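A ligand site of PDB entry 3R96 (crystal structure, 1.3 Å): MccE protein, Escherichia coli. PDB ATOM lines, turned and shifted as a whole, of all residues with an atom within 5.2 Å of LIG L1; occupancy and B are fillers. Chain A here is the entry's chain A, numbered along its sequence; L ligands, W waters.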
ATOM      1  N   LEU A  35      17.930 -24.543  -5.792  1.00  0.00           N
ATOM      2  CA  LEU A  35      16.495 -24.795  -5.876  1.00  0.00           C
ATOM      3  C   LEU A  35      16.049 -25.786  -4.803  1.00  0.00           C
ATOM      4  O   LEU A  35      15.066 -25.535  -4.092  1.00  0.00           O
ATOM      5  CB  LEU A  35      16.125 -25.301  -7.270  1.00  0.00           C
ATOM      6  CG  LEU A  35      14.637 -25.590  -7.514  1.00  0.00           C
ATOM      7  CD1 LEU A  35      13.803 -24.309  -7.544  1.00  0.00           C
ATOM      8  CD2 LEU A  35      14.450 -26.359  -8.808  1.00  0.00           C
ATOM      9  N   ILE A  39      13.393 -25.059  -1.674  1.00  0.00           N
ATOM     10  CA  ILE A  39      12.202 -25.872  -1.436  1.00  0.00           C
ATOM     11  C   ILE A  39      12.236 -26.449  -0.023  1.00  0.00           C
ATOM     12  O   ILE A  39      11.257 -26.383   0.716  1.00  0.00           O
ATOM     13  CB  ILE A  39      12.061 -27.006  -2.469  1.00  0.00           C
ATOM     14  CG1 ILE A  39      11.800 -26.425  -3.859  1.00  0.00           C
ATOM     15  CG2 ILE A  39      10.929 -27.948  -2.084  1.00  0.00           C
ATOM     16  CD1 ILE A  39      12.083 -27.402  -4.989  1.00  0.00           C
ATOM     17  N   MET A  50       0.376 -26.798  -2.136  1.00  0.00           N
ATOM     18  CA  MET A  50       0.838 -27.527  -3.325  1.00  0.00           C
ATOM     19  C   MET A  50       1.081 -28.984  -2.954  1.00  0.00           C
ATOM     20  O   MET A  50       1.388 -29.285  -1.798  1.00  0.00           O
ATOM     21  CB  MET A  50       2.109 -26.878  -3.892  1.00  0.00           C
ATOM     22  CG  MET A  50       1.939 -25.421  -4.320  1.00  0.00           C
ATOM     23  SD  MET A  50       3.426 -24.649  -4.990  1.00  0.00           S
ATOM     24  CE  MET A  50       4.519 -24.649  -3.570  1.00  0.00           C
ATOM     25  N   ALA A  51       0.964 -29.881  -3.940  1.00  0.00           N
ATOM     26  CA  ALA A  51       0.948 -31.338  -3.716  1.00  0.00           C
ATOM     27  C   ALA A  51       2.279 -32.049  -3.961  1.00  0.00           C
ATOM     28  O   ALA A  51       2.392 -33.247  -3.686  1.00  0.00           O
ATOM     29  CB  ALA A  51      -0.114 -31.985  -4.601  1.00  0.00           C
ATOM     30  N   TRP A  52       3.239 -31.348  -4.551  1.00  0.00           N
ATOM     31  CA  TRP A  52       4.554 -31.912  -4.851  1.00  0.00           C
ATOM     32  C   TRP A  52       5.635 -31.681  -3.779  1.00  0.00           C
ATOM     33  O   TRP A  52       6.540 -32.498  -3.680  1.00  0.00           O
ATOM     34  CB  TRP A  52       5.046 -31.421  -6.233  1.00  0.00           C
ATOM     35  CG  TRP A  52       5.077 -29.931  -6.333  1.00  0.00           C
ATOM     36  CD1 TRP A  52       4.085 -29.119  -6.807  1.00  0.00           C
ATOM     37  CD2 TRP A  52       6.136 -29.064  -5.896  1.00  0.00           C
ATOM     38  NE1 TRP A  52       4.465 -27.798  -6.698  1.00  0.00           N
ATOM     39  CE2 TRP A  52       5.722 -27.734  -6.150  1.00  0.00           C
ATOM     40  CE3 TRP A  52       7.405 -29.273  -5.327  1.00  0.00           C
ATOM     41  CZ2 TRP A  52       6.506 -26.627  -5.843  1.00  0.00           C
ATOM     42  CZ3 TRP A  52       8.186 -28.171  -5.033  1.00  0.00           C
ATOM     43  CH2 TRP A  52       7.736 -26.870  -5.290  1.00  0.00           C
ATOM     44  N   VAL A  56       9.670 -33.816  -2.090  1.00  0.00           N
ATOM     45  CA  VAL A  56      11.008 -33.318  -2.409  1.00  0.00           C
ATOM     46  C   VAL A  56      11.920 -33.584  -1.221  1.00  0.00           C
ATOM     47  O   VAL A  56      11.935 -32.816  -0.260  1.00  0.00           O
ATOM     48  CB  VAL A  56      11.003 -31.818  -2.786  1.00  0.00           C
ATOM     49  CG1 VAL A  56      12.415 -31.345  -3.129  1.00  0.00           C
ATOM     50  CG2 VAL A  56      10.067 -31.565  -3.956  1.00  0.00           C
ATOM     51  N   PHE A  65      13.425 -32.886 -11.594  1.00  0.00           N
ATOM     52  CA  PHE A  65      12.510 -31.817 -11.980  1.00  0.00           C
ATOM     53  C   PHE A  65      13.111 -30.918 -13.061  1.00  0.00           C
ATOM     54  O   PHE A  65      12.442 -30.564 -14.032  1.00  0.00           O
ATOM     55  CB  PHE A  65      12.112 -30.989 -10.753  1.00  0.00           C
ATOM     56  CG  PHE A  65      11.299 -29.777 -11.096  1.00  0.00           C
ATOM     57  CD1 PHE A  65       9.965 -29.910 -11.488  1.00  0.00           C
ATOM     58  CD2 PHE A  65      11.852 -28.503 -11.042  1.00  0.00           C
ATOM     59  CE1 PHE A  65       9.204 -28.788 -11.823  1.00  0.00           C
ATOM     60  CE2 PHE A  65      11.104 -27.376 -11.375  1.00  0.00           C
ATOM     61  CZ  PHE A  65       9.778 -27.533 -11.767  1.00  0.00           C
ATOM     62  N   ILE A  80       8.896 -23.445 -18.062  1.00  0.00           N
ATOM     63  CA  ILE A  80       9.275 -23.442 -16.655  1.00  0.00           C
ATOM     64  C   ILE A  80      10.457 -22.492 -16.500  1.00  0.00           C
ATOM     65  O   ILE A  80      11.457 -22.617 -17.204  1.00  0.00           O
ATOM     66  CB  ILE A  80       9.680 -24.862 -16.174  1.00  0.00           C
ATOM     67  CG1 ILE A  80       8.628 -25.908 -16.572  1.00  0.00           C
ATOM     68  CG2 ILE A  80       9.977 -24.875 -14.678  1.00  0.00           C
ATOM     69  CD1 ILE A  80       7.211 -25.647 -16.063  1.00  0.00           C
ATOM     70  N   VAL A  92       9.710 -20.128  -8.619  1.00  0.00           N
ATOM     71  CA  VAL A  92       9.432 -20.599  -9.964  1.00  0.00           C
ATOM     72  C   VAL A  92       8.201 -19.873 -10.501  1.00  0.00           C
ATOM     73  O   VAL A  92       7.248 -19.625  -9.749  1.00  0.00           O
ATOM     74  CB  VAL A  92       9.186 -22.144  -9.985  1.00  0.00           C
ATOM     75  CG1 VAL A  92       8.816 -22.650 -11.379  1.00  0.00           C
ATOM     76  CG2 VAL A  92      10.418 -22.895  -9.485  1.00  0.00           C
ATOM     77  N   VAL A  93       8.229 -19.497 -11.778  1.00  0.00           N
ATOM     78  CA  VAL A  93       7.019 -19.089 -12.473  1.00  0.00           C
ATOM     79  C   VAL A  93       6.952 -19.872 -13.775  1.00  0.00           C
ATOM     80  O   VAL A  93       7.978 -20.150 -14.393  1.00  0.00           O
ATOM     81  CB  VAL A  93       6.953 -17.560 -12.753  1.00  0.00           C
ATOM     82  CG1 VAL A  93       6.727 -16.759 -11.503  1.00  0.00           C
ATOM     83  CG2 VAL A  93       8.163 -17.065 -13.579  1.00  0.00           C
ATOM     84  N   SER A  94       5.748 -20.245 -14.181  1.00  0.00           N
ATOM     85  CA  SER A  94       5.621 -21.161 -15.305  1.00  0.00           C
ATOM     86  C   SER A  94       4.355 -20.990 -16.118  1.00  0.00           C
ATOM     87  O   SER A  94       3.322 -20.540 -15.599  1.00  0.00           O
ATOM     88  CB  SER A  94       5.663 -22.603 -14.805  1.00  0.00           C
ATOM     89  OG  SER A  94       4.680 -22.777 -13.804  1.00  0.00           O
ATOM     90  N   ASN A  96       2.593 -23.892 -16.978  1.00  0.00           N
ATOM     91  CA  ASN A  96       2.617 -25.332 -16.716  1.00  0.00           C
ATOM     92  C   ASN A  96       2.076 -26.143 -17.890  1.00  0.00           C
ATOM     93  O   ASN A  96       2.502 -27.275 -18.118  1.00  0.00           O
ATOM     94  CB  ASN A  96       1.839 -25.668 -15.450  1.00  0.00           C
ATOM     95  CG  ASN A  96       2.652 -25.469 -14.182  1.00  0.00           C
ATOM     96  OD1 ASN A  96       3.886 -25.553 -14.186  1.00  0.00           O
ATOM     97  ND2 ASN A  96       1.959 -25.268 -13.068  1.00  0.00           N
ATOM     98  N   GLY A 108       1.502 -21.087 -13.358  1.00  0.00           N
ATOM     99  CA  GLY A 108       1.767 -21.494 -11.977  1.00  0.00           C
ATOM    100  C   GLY A 108       2.918 -20.689 -11.404  1.00  0.00           C
ATOM    101  O   GLY A 108       3.706 -20.083 -12.140  1.00  0.00           O
ATOM    102  N   TYR A 109       3.022 -20.684 -10.071  1.00  0.00           N
ATOM    103  CA  TYR A 109       4.068 -19.900  -9.401  1.00  0.00           C
ATOM    104  C   TYR A 109       4.236 -20.289  -7.948  1.00  0.00           C
ATOM    105  O   TYR A 109       3.289 -20.754  -7.301  1.00  0.00           O
ATOM    106  CB  TYR A 109       3.782 -18.394  -9.500  1.00  0.00           C
ATOM    107  CG  TYR A 109       2.325 -18.006  -9.329  1.00  0.00           C
ATOM    108  CD1 TYR A 109       1.740 -17.922  -8.069  1.00  0.00           C
ATOM    109  CD2 TYR A 109       1.545 -17.709 -10.437  1.00  0.00           C
ATOM    110  CE1 TYR A 109       0.399 -17.567  -7.921  1.00  0.00           C
ATOM    111  CE2 TYR A 109       0.222 -17.334 -10.301  1.00  0.00           C
ATOM    112  CZ  TYR A 109      -0.356 -17.265  -9.053  1.00  0.00           C
ATOM    113  OH  TYR A 109      -1.681 -16.908  -8.949  1.00  0.00           O
ATOM    114  N   TRP A 110       5.439 -20.066  -7.444  1.00  0.00           N
ATOM    115  CA  TRP A 110       5.691 -20.063  -6.013  1.00  0.00           C
ATOM    116  C   TRP A 110       6.911 -19.221  -5.683  1.00  0.00           C
ATOM    117  O   TRP A 110       7.790 -19.052  -6.539  1.00  0.00           O
ATOM    118  CB  TRP A 110       5.849 -21.475  -5.459  1.00  0.00           C
ATOM    119  CG  TRP A 110       7.021 -22.297  -5.925  1.00  0.00           C
ATOM    120  CD1 TRP A 110       6.992 -23.282  -6.866  1.00  0.00           C
ATOM    121  CD2 TRP A 110       8.364 -22.297  -5.395  1.00  0.00           C
ATOM    122  NE1 TRP A 110       8.233 -23.875  -6.988  1.00  0.00           N
ATOM    123  CE2 TRP A 110       9.086 -23.292  -6.088  1.00  0.00           C
ATOM    124  CE3 TRP A 110       9.027 -21.544  -4.416  1.00  0.00           C
ATOM    125  CZ2 TRP A 110      10.438 -23.551  -5.831  1.00  0.00           C
ATOM    126  CZ3 TRP A 110      10.360 -21.814  -4.158  1.00  0.00           C
ATOM    127  CH2 TRP A 110      11.051 -22.802  -4.861  1.00  0.00           C
ATOM    128  N   GLU A 171      -9.015 -29.604  -7.529  1.00  0.00           N
ATOM    129  CA  GLU A 171      -7.610 -29.770  -7.166  1.00  0.00           C
ATOM    130  C   GLU A 171      -7.476 -30.595  -5.897  1.00  0.00           C
ATOM    131  O   GLU A 171      -8.074 -30.265  -4.866  1.00  0.00           O
ATOM    132  CB  GLU A 171      -6.897 -28.421  -7.018  1.00  0.00           C
ATOM    133  CG  GLU A 171      -5.403 -28.592  -6.816  1.00  0.00           C
ATOM    134  CD  GLU A 171      -4.619 -27.289  -6.823  1.00  0.00           C
ATOM    135  OE1 GLU A 171      -5.167 -26.231  -7.201  1.00  0.00           O
ATOM    136  OE2 GLU A 171      -3.419 -27.331  -6.453  1.00  0.00           O
HETATM  137  P1  LIG L   1       1.251 -26.292  -8.766  1.00  0.00           P
HETATM  138  O1  LIG L   1       0.755 -27.176  -9.890  1.00  0.00           O
HETATM  139  O2  LIG L   1       0.180 -25.305  -8.321  1.00  0.00           O
HETATM  140  O3  LIG L   1       1.925 -27.006  -7.635  1.00  0.00           O
HETATM  141  O4  LIG L   1       2.399 -25.453  -9.528  1.00  0.00           O
HETATM  142  C1  LIG L   1       2.885 -24.270  -8.904  1.00  0.00           C
HETATM  143  C2  LIG L   1       4.348 -24.047  -9.300  1.00  0.00           C
HETATM  144  O5  LIG L   1       5.175 -25.077  -8.745  1.00  0.00           O
HETATM  145  C3  LIG L   1       4.598 -24.026 -10.801  1.00  0.00           C
HETATM  146  O6  LIG L   1       5.391 -22.862 -11.059  1.00  0.00           O
HETATM  147  C4  LIG L   1       5.383 -25.301 -11.052  1.00  0.00           C
HETATM  148  O7  LIG L   1       6.277 -25.221 -12.165  1.00  0.00           O
HETATM  149  C5  LIG L   1       6.123 -25.447  -9.744  1.00  0.00           C
HETATM  150  N1  LIG L   1       6.610 -26.809  -9.456  1.00  0.00           N
HETATM  151  C6  LIG L   1       5.929 -27.956  -9.646  1.00  0.00           C
HETATM  152  N2  LIG L   1       6.664 -29.019  -9.282  1.00  0.00           N
HETATM  153  C7  LIG L   1       7.836 -28.550  -8.845  1.00  0.00           C
HETATM  154  C8  LIG L   1       9.076 -29.139  -8.319  1.00  0.00           C
HETATM  155  N3  LIG L   1       9.176 -30.476  -8.187  1.00  0.00           N
HETATM  156  N4  LIG L   1      10.079 -28.306  -7.994  1.00  0.00           N
HETATM  157  C9  LIG L   1       9.962 -26.966  -8.122  1.00  0.00           C
HETATM  158  N5  LIG L   1       8.859 -26.357  -8.604  1.00  0.00           N
HETATM  159  C10 LIG L   1       7.799 -27.096  -8.961  1.00  0.00           C
HETATM  160  N1  LG2 L   2       4.532  -4.636  -7.129  1.00  0.00           N
HETATM  161  C1  LG2 L   2       3.459  -5.309  -6.664  1.00  0.00           C
HETATM  162  N2  LG2 L   2       3.361  -5.688  -5.376  1.00  0.00           N
HETATM  163  C2  LG2 L   2       4.355  -5.367  -4.507  1.00  0.00           C
HETATM  164  C3  LG2 L   2       5.470  -4.666  -4.963  1.00  0.00           C
HETATM  165  C4  LG2 L   2       5.545  -4.307  -6.291  1.00  0.00           C
HETATM  166  N3  LG2 L   2       6.625  -3.624  -6.731  1.00  0.00           N
HETATM  167  N4  LG2 L   2       6.310  -4.487  -3.928  1.00  0.00           N
HETATM  168  C5  LG2 L   2       5.726  -5.056  -2.851  1.00  0.00           C
HETATM  169  N5  LG2 L   2       4.534  -5.568  -3.195  1.00  0.00           N
HETATM  170  C6  LG2 L   2       3.689  -6.366  -2.274  1.00  0.00           C
HETATM  171  C7  LG2 L   2       2.187  -6.261  -2.330  1.00  0.00           C
HETATM  172  O1  LG2 L   2       1.728  -5.236  -1.457  1.00  0.00           O
HETATM  173  C8  LG2 L   2       1.748  -7.644  -1.883  1.00  0.00           C
HETATM  174  O2  LG2 L   2       1.969  -7.807  -0.472  1.00  0.00           O
HETATM  175  P1  LG2 L   2       0.812  -8.201   0.590  1.00  0.00           P
HETATM  176  O3  LG2 L   2       1.432  -7.880   1.926  1.00  0.00           O
HETATM  177  O4  LG2 L   2       0.509  -9.671   0.389  1.00  0.00           O
HETATM  178  O5  LG2 L   2      -0.353  -7.326   0.219  1.00  0.00           O
HETATM  179  C9  LG2 L   2       2.778  -8.541  -2.534  1.00  0.00           C
HETATM  180  O6  LG2 L   2       3.950  -7.737  -2.670  1.00  0.00           O
HETATM  181  C10 LG2 L   2       2.317  -9.071  -3.888  1.00  0.00           C
HETATM  182  O7  LG2 L   2       3.393  -9.772  -4.496  1.00  0.00           O
HETATM  183  P2  LG2 L   2       3.129 -10.877  -5.644  1.00  0.00           P
HETATM  184  O8  LG2 L   2       1.712 -10.795  -6.133  1.00  0.00           O
HETATM  185  O9  LG2 L   2       4.239 -10.807  -6.642  1.00  0.00           O
HETATM  186  O10 LG2 L   2       3.279 -12.292  -4.868  1.00  0.00           O
HETATM  187  P3  LG2 L   2       3.465 -12.626  -3.301  1.00  0.00           P
HETATM  188  O11 LG2 L   2       4.809 -12.172  -2.822  1.00  0.00           O
HETATM  189  O12 LG2 L   2       2.250 -12.183  -2.563  1.00  0.00           O
HETATM  190  O13 LG2 L   2       3.468 -14.221  -3.409  1.00  0.00           O
HETATM  191  C11 LG2 L   2       2.540 -16.411  -3.886  1.00  0.00           C
HETATM  192  C12 LG2 L   2       2.262 -14.919  -3.754  1.00  0.00           C
HETATM  193  C13 LG2 L   2       1.228 -17.111  -4.226  1.00  0.00           C
HETATM  194  C14 LG2 L   2       3.559 -16.598  -5.015  1.00  0.00           C
HETATM  195  C15 LG2 L   2       3.100 -16.917  -2.552  1.00  0.00           C
HETATM  196  O14 LG2 L   2       2.164 -16.626  -1.516  1.00  0.00           O
HETATM  197  C16 LG2 L   2       3.451 -18.382  -2.533  1.00  0.00           C
HETATM  198  O15 LG2 L   2       4.448 -18.804  -3.109  1.00  0.00           O
HETATM  199  N6  LG2 L   2       2.635 -19.212  -1.880  1.00  0.00           N
HETATM  200  C17 LG2 L   2       2.792 -20.660  -1.695  1.00  0.00           C
HETATM  201  C18 LG2 L   2       2.764 -21.404  -3.022  1.00  0.00           C
HETATM  202  C19 LG2 L   2       1.443 -21.185  -3.724  1.00  0.00           C
HETATM  203  O16 LG2 L   2       0.388 -21.155  -3.108  1.00  0.00           O
HETATM  204  N7  LG2 L   2       1.483 -21.016  -5.045  1.00  0.00           N
HETATM  205  C20 LG2 L   2       0.337 -20.781  -5.914  1.00  0.00           C
HETATM  206  C21 LG2 L   2      -0.328 -22.113  -6.276  1.00  0.00           C
HETATM  207  S1  LG2 L   2      -1.691 -21.785  -7.347  1.00  0.00           S
HETATM  208  C22 LG2 L   2      -0.918 -21.381  -8.803  1.00  0.00           C
HETATM  209  O17 LG2 L   2       0.277 -21.587  -9.007  1.00  0.00           O
HETATM  210  C23 LG2 L   2      -1.735 -20.726  -9.883  1.00  0.00           C
HETATM  211  O   HOH W   1      11.223 -32.361  -7.338  1.00  0.00           O
HETATM  212  O   HOH W   2       2.883 -28.412 -10.503  1.00  0.00           O
HETATM  213  O   HOH W   3       5.634 -31.484  -9.841  1.00  0.00           O
HETATM  214  O   HOH W   4      -1.435 -25.579  -6.084  1.00  0.00           O
HETATM  215  O   HOH W   5       7.567 -32.934  -8.505  1.00  0.00           O
HETATM  216  O   HOH W   6       6.313 -27.722 -13.308  1.00  0.00           O
HETATM  217  O   HOH W   7       0.539 -29.025  -6.620  1.00  0.00           O
HETATM  218  O   HOH W   8      12.413 -29.828  -7.174  1.00  0.00           O
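Water W7 lies within hydrogen-bond range of an oxygen (O3) of LIG L1 and the backbone NH of Ala 51. Water W6 bridges O7 of LIG L1 (2.8 Å) and OD1 of Asn 96 (3.4 Å). Water W4 lies within hydrogen-bond range of OE2 of Glu 171 (2.7 Å) and O2 of LIG L1 (2.8 Å).
An oxygen (O3) of LIG L1 sits at hydrogen-bond distance from the indole nitrogen (NE1) of Trp 52. An oxygen (O6) of LIG L1 is in hydrogen-bond range of the side-chain hydroxyl (OG) of Ser 94 (2.8 Å). N5 of LIG L1 sits at hydrogen-bond distance from NE1 of Trp 110 (3.0 Å). The side-chain amide oxygen of Asn 96 lies within hydrogen-bond range of an oxygen (O7) of LIG L1, 3.1 Å away. O of Gly 108 lies close to O6 of LIG L1 (3.4 Å). N of Tyr 109 lies within hydrogen-bond range of O6 of LIG L1 (3.4 Å). The backbone NH (N) of Tyr 109 sits at hydrogen-bond distance from an oxygen (O17) of LG2 L2, at 3.1 Å. A nitrogen (N7) of LG2 L2 sits at hydrogen-bond distance from the backbone carbonyl oxygen (O) of Tyr 109 (2.9 Å).
The indole nitrogen (NE1) of Trp 52 sits at hydrogen-bond distance from the side-chain sulfur (SD) of Met 50 (3.7 Å). OG of Ser 94 lies within hydrogen-bond range of OD1 of Asn 96, at 2.9 Å. N of Ser 94 sits at hydrogen-bond distance from O of Gly 108, at 2.9 Å. The backbone NH (N) of Trp 110 lies within hydrogen-bond range of the backbone carbonyl oxygen (O) of Val 92 (3.0 Å).
Residues that only touch LIG L1: Ile 39 (3.7 Å), Met 50 (3.7 Å), Phe 65 (3.3 Å) and Val 92 (3.4 Å). Hydrophobic or aromatic side chains within 4 Å of LIG L1: Ile 39, Met 50, Trp 52, Phe 65, Val 92 and Trp 110. Of the 16 residues printed, 10 come within 4 Å of LIG L1.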
